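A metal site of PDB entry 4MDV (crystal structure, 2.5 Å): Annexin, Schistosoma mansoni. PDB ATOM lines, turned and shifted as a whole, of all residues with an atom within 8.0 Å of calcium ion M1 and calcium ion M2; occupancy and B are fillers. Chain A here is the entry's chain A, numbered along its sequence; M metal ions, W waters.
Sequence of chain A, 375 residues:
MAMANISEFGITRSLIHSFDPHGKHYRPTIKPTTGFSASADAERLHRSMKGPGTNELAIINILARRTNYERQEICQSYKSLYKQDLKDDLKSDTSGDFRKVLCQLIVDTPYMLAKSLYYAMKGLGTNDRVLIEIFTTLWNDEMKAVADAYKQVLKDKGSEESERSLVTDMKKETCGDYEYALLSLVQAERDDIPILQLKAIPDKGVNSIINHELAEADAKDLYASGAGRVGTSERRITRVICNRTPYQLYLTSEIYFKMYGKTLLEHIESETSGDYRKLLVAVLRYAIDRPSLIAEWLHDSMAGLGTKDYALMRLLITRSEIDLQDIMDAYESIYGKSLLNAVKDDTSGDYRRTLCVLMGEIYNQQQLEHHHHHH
Gly 304 touches calcium ion M1 (O to CA, 3.2 Å). Along chain A the residues within 4 Å of calcium ion M1 span positions 302 to 346. The nearest printed residue that does not touch calcium ion M1 is Ala 303 (4.4 Å).
Within 4 Å of calcium ion M2: Gly 306 and Asp 346.
The side-chain carboxylate (OD1) of Asp 346 binds calcium ion M1 (2.4 Å). The backbone carbonyl oxygen (O) of Leu 305 binds calcium ion M1. OD2 of Asp 346 binds calcium ion M1 (2.5 Å). The backbone carbonyl oxygen (O) of Met 302 binds calcium ion M1. Calcium ion M1 has four donor atoms within binding distance.
O of Asp 346 binds calcium ion M2 (2.5 Å). Calcium ion M2 is bound by water W1, 2.6 Å away. The backbone carbonyl oxygen (O) of Gly 306 is bound to calcium ion M2, at 2.8 Å. Calcium ion M2 has three donor atoms within binding distance.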
ATOM      1  N   ASP A  97      14.539  -7.246  29.682  1.00  0.00           N
ATOM      2  CA  ASP A  97      13.321  -6.866  28.985  1.00  0.00           C
ATOM      3  C   ASP A  97      13.554  -5.575  28.220  1.00  0.00           C
ATOM      4  O   ASP A  97      12.964  -5.344  27.155  1.00  0.00           O
ATOM      5  CB  ASP A  97      12.172  -6.697  29.971  1.00  0.00           C
ATOM      6  CG  ASP A  97      11.711  -8.013  30.562  1.00  0.00           C
ATOM      7  OD1 ASP A  97      11.532  -8.988  29.794  1.00  0.00           O
ATOM      8  OD2 ASP A  97      11.546  -8.072  31.804  1.00  0.00           O
ATOM      9  N   HIS A 299      -5.290  -6.292  25.426  1.00  0.00           N
ATOM     10  CA  HIS A 299      -5.774  -6.897  26.659  1.00  0.00           C
ATOM     11  C   HIS A 299      -5.319  -8.338  26.714  1.00  0.00           C
ATOM     12  O   HIS A 299      -4.842  -8.841  27.754  1.00  0.00           O
ATOM     13  CB  HIS A 299      -7.294  -6.834  26.686  1.00  0.00           C
ATOM     14  CG  HIS A 299      -7.900  -7.366  27.945  1.00  0.00           C
ATOM     15  ND1 HIS A 299      -7.832  -6.689  29.141  1.00  0.00           N
ATOM     16  CD2 HIS A 299      -8.588  -8.503  28.192  1.00  0.00           C
ATOM     17  CE1 HIS A 299      -8.469  -7.382  30.072  1.00  0.00           C
ATOM     18  NE2 HIS A 299      -8.935  -8.490  29.521  1.00  0.00           N
ATOM     19  N   ASP A 300      -5.459  -9.009  25.589  1.00  0.00           N
ATOM     20  CA  ASP A 300      -5.133 -10.413  25.513  1.00  0.00           C
ATOM     21  C   ASP A 300      -3.619 -10.664  25.632  1.00  0.00           C
ATOM     22  O   ASP A 300      -3.208 -11.681  26.184  1.00  0.00           O
ATOM     23  CB  ASP A 300      -5.746 -11.005  24.257  1.00  0.00           C
ATOM     24  CG  ASP A 300      -7.257 -10.899  24.260  1.00  0.00           C
ATOM     25  OD1 ASP A 300      -7.819 -10.440  25.294  1.00  0.00           O
ATOM     26  OD2 ASP A 300      -7.911 -11.263  23.267  1.00  0.00           O
ATOM     27  N   SER A 301      -2.807  -9.709  25.158  1.00  0.00           N
ATOM     28  CA  SER A 301      -1.366  -9.843  25.299  1.00  0.00           C
ATOM     29  C   SER A 301      -0.953  -9.745  26.780  1.00  0.00           C
ATOM     30  O   SER A 301       0.153 -10.141  27.138  1.00  0.00           O
ATOM     31  CB  SER A 301      -0.615  -8.788  24.475  1.00  0.00           C
ATOM     32  OG  SER A 301      -0.579  -7.528  25.151  1.00  0.00           O
ATOM     33  N   MET A 302      -1.826  -9.200  27.619  1.00  0.00           N
ATOM     34  CA  MET A 302      -1.537  -9.037  29.037  1.00  0.00           C
ATOM     35  C   MET A 302      -2.241 -10.061  29.947  1.00  0.00           C
ATOM     36  O   MET A 302      -1.778 -10.314  31.046  1.00  0.00           O
ATOM     37  CB  MET A 302      -1.836  -7.604  29.502  1.00  0.00           C
ATOM     38  CG  MET A 302      -0.826  -6.619  28.992  1.00  0.00           C
ATOM     39  SD  MET A 302      -1.291  -4.904  29.275  1.00  0.00           S
ATOM     40  CE  MET A 302      -2.825  -4.808  28.335  1.00  0.00           C
ATOM     41  N   ALA A 303      -3.348 -10.633  29.470  1.00  0.00           N
ATOM     42  CA  ALA A 303      -4.079 -11.657  30.220  1.00  0.00           C
ATOM     43  C   ALA A 303      -3.178 -12.712  30.838  1.00  0.00           C
ATOM     44  O   ALA A 303      -2.189 -13.155  30.229  1.00  0.00           O
ATOM     45  CB  ALA A 303      -5.118 -12.348  29.310  1.00  0.00           C
ATOM     46  N   GLY A 304      -3.547 -13.131  32.053  1.00  0.00           N
ATOM     47  CA  GLY A 304      -2.834 -14.167  32.773  1.00  0.00           C
ATOM     48  C   GLY A 304      -1.529 -13.629  33.321  1.00  0.00           C
ATOM     49  O   GLY A 304      -1.508 -12.988  34.360  1.00  0.00           O
ATOM     50  N   LEU A 305      -0.438 -13.885  32.624  1.00  0.00           N
ATOM     51  CA  LEU A 305       0.857 -13.399  33.085  1.00  0.00           C
ATOM     52  C   LEU A 305       1.633 -12.584  32.041  1.00  0.00           C
ATOM     53  O   LEU A 305       1.083 -11.810  31.261  1.00  0.00           O
ATOM     54  CB  LEU A 305       1.724 -14.531  33.630  1.00  0.00           C
ATOM     55  N   GLY A 306       2.946 -12.796  32.040  1.00  0.00           N
ATOM     56  CA  GLY A 306       3.934 -11.988  31.345  1.00  0.00           C
ATOM     57  C   GLY A 306       3.685 -11.170  30.084  1.00  0.00           C
ATOM     58  O   GLY A 306       2.981 -10.172  30.151  1.00  0.00           O
ATOM     59  N   THR A 307       4.227 -11.530  28.933  1.00  0.00           N
ATOM     60  CA  THR A 307       4.306 -12.829  28.299  1.00  0.00           C
ATOM     61  C   THR A 307       2.981 -13.123  27.611  1.00  0.00           C
ATOM     62  O   THR A 307       2.259 -14.039  27.990  1.00  0.00           O
ATOM     63  CB  THR A 307       4.778 -14.020  29.196  1.00  0.00           C
ATOM     64  N   LYS A 308       2.603 -12.148  26.801  1.00  0.00           N
ATOM     65  CA  LYS A 308       2.712 -12.214  25.359  1.00  0.00           C
ATOM     66  C   LYS A 308       3.513 -10.922  25.108  1.00  0.00           C
ATOM     67  O   LYS A 308       3.051 -10.001  24.434  1.00  0.00           O
ATOM     68  CB  LYS A 308       1.356 -12.204  24.676  1.00  0.00           C
ATOM     69  CG  LYS A 308       0.889 -13.568  24.186  1.00  0.00           C
ATOM     70  CD  LYS A 308      -0.007 -14.253  25.191  1.00  0.00           C
ATOM     71  CE  LYS A 308      -0.911 -15.293  24.530  1.00  0.00           C
ATOM     72  NZ  LYS A 308      -2.161 -14.706  23.936  1.00  0.00           N
ATOM     73  N   ASP A 309       4.708 -10.847  25.716  1.00  0.00           N
ATOM     74  CA  ASP A 309       5.502  -9.610  25.710  1.00  0.00           C
ATOM     75  C   ASP A 309       5.747  -9.063  24.315  1.00  0.00           C
ATOM     76  O   ASP A 309       5.737  -7.835  24.100  1.00  0.00           O
ATOM     77  CB  ASP A 309       6.855  -9.840  26.382  1.00  0.00           C
ATOM     78  CG  ASP A 309       6.775  -9.833  27.888  1.00  0.00           C
ATOM     79  OD1 ASP A 309       6.553  -8.745  28.461  1.00  0.00           O
ATOM     80  OD2 ASP A 309       6.936 -10.916  28.489  1.00  0.00           O
ATOM     81  N   LEU A 312       2.639  -7.492  22.772  1.00  0.00           N
ATOM     82  CA  LEU A 312       2.446  -6.192  23.427  1.00  0.00           C
ATOM     83  C   LEU A 312       3.379  -5.132  22.822  1.00  0.00           C
ATOM     84  O   LEU A 312       2.921  -4.072  22.427  1.00  0.00           O
ATOM     85  CB  LEU A 312       2.672  -6.320  24.940  1.00  0.00           C
ATOM     86  CG  LEU A 312       2.567  -4.988  25.682  1.00  0.00           C
ATOM     87  CD1 LEU A 312       1.176  -4.395  25.522  1.00  0.00           C
ATOM     88  CD2 LEU A 312       2.898  -5.162  27.167  1.00  0.00           C
ATOM     89  N   ALA A 342      -2.954  -0.677  32.654  1.00  0.00           N
ATOM     90  CA  ALA A 342      -2.901  -2.125  32.445  1.00  0.00           C
ATOM     91  C   ALA A 342      -1.471  -2.508  32.125  1.00  0.00           C
ATOM     92  O   ALA A 342      -0.957  -3.536  32.586  1.00  0.00           O
ATOM     93  CB  ALA A 342      -3.819  -2.559  31.361  1.00  0.00           C
ATOM     94  N   VAL A 343      -0.818  -1.663  31.341  1.00  0.00           N
ATOM     95  CA  VAL A 343       0.571  -1.909  30.930  1.00  0.00           C
ATOM     96  C   VAL A 343       1.497  -1.754  32.138  1.00  0.00           C
ATOM     97  O   VAL A 343       2.394  -2.582  32.366  1.00  0.00           O
ATOM     98  CB  VAL A 343       1.002  -0.950  29.748  1.00  0.00           C
ATOM     99  CG1 VAL A 343       2.505  -0.939  29.535  1.00  0.00           C
ATOM    100  CG2 VAL A 343       0.285  -1.313  28.455  1.00  0.00           C
ATOM    101  N   ASP A 345       0.767  -2.316  35.127  1.00  0.00           N
ATOM    102  CA  ASP A 345       0.551  -3.414  36.047  1.00  0.00           C
ATOM    103  C   ASP A 345       1.131  -4.740  35.568  1.00  0.00           C
ATOM    104  O   ASP A 345       1.299  -5.670  36.357  1.00  0.00           O
ATOM    105  CB  ASP A 345      -0.914  -3.596  36.324  1.00  0.00           C
ATOM    106  CG  ASP A 345      -1.496  -2.417  37.066  1.00  0.00           C
ATOM    107  OD1 ASP A 345      -0.687  -1.557  37.493  1.00  0.00           O
ATOM    108  OD2 ASP A 345      -2.733  -2.350  37.199  1.00  0.00           O
ATOM    109  N   ASP A 346       1.407  -4.830  34.277  1.00  0.00           N
ATOM    110  CA  ASP A 346       1.866  -6.100  33.736  1.00  0.00           C
ATOM    111  C   ASP A 346       3.364  -6.117  33.464  1.00  0.00           C
ATOM    112  O   ASP A 346       3.924  -7.152  33.173  1.00  0.00           O
ATOM    113  CB  ASP A 346       1.117  -6.462  32.443  1.00  0.00           C
ATOM    114  CG  ASP A 346       0.531  -7.845  32.508  1.00  0.00           C
ATOM    115  OD1 ASP A 346      -0.032  -8.185  33.569  1.00  0.00           O
ATOM    116  OD2 ASP A 346       0.628  -8.606  31.518  1.00  0.00           O
ATOM    117  N   THR A 347       4.034  -4.978  33.569  1.00  0.00           N
ATOM    118  CA  THR A 347       5.436  -4.925  33.192  1.00  0.00           C
ATOM    119  C   THR A 347       6.251  -4.120  34.206  1.00  0.00           C
ATOM    120  O   THR A 347       5.694  -3.542  35.149  1.00  0.00           O
ATOM    121  CB  THR A 347       5.630  -4.356  31.726  1.00  0.00           C
ATOM    122  OG1 THR A 347       5.196  -2.994  31.657  1.00  0.00           O
ATOM    123  CG2 THR A 347       4.815  -5.162  30.702  1.00  0.00           C
ATOM    124  N   SER A 348       7.565  -4.096  34.034  1.00  0.00           N
ATOM    125  CA  SER A 348       8.414  -3.284  34.896  1.00  0.00           C
ATOM    126  C   SER A 348       9.728  -2.902  34.262  1.00  0.00           C
ATOM    127  O   SER A 348      10.014  -3.238  33.112  1.00  0.00           O
ATOM    128  CB  SER A 348       8.668  -3.913  36.281  1.00  0.00           C
ATOM    129  OG  SER A 348       8.646  -5.327  36.240  1.00  0.00           O
ATOM    130  N   TYR A 351      11.919  -1.450  30.494  1.00  0.00           N
ATOM    131  CA  TYR A 351      10.925  -2.004  29.592  1.00  0.00           C
ATOM    132  C   TYR A 351       9.539  -1.342  29.757  1.00  0.00           C
ATOM    133  O   TYR A 351       8.941  -0.920  28.766  1.00  0.00           O
ATOM    134  CB  TYR A 351      10.855  -3.518  29.761  1.00  0.00           C
ATOM    135  CG  TYR A 351       9.744  -4.227  29.005  1.00  0.00           C
ATOM    136  CD1 TYR A 351       9.610  -4.116  27.622  1.00  0.00           C
ATOM    137  CD2 TYR A 351       8.850  -5.043  29.669  1.00  0.00           C
ATOM    138  CE1 TYR A 351       8.600  -4.770  26.940  1.00  0.00           C
ATOM    139  CE2 TYR A 351       7.853  -5.702  29.017  1.00  0.00           C
ATOM    140  CZ  TYR A 351       7.724  -5.567  27.653  1.00  0.00           C
ATOM    141  OH  TYR A 351       6.710  -6.240  27.012  1.00  0.00           O
HETATM  142 CA    CA M   1      -0.105 -10.478  32.982  1.00  0.00          CA
HETATM  143 CA    CA M   2       4.295  -9.525  32.535  1.00  0.00          CA
HETATM  144  O   HOH W   1       3.028  -9.885  34.833  1.00  0.00           O
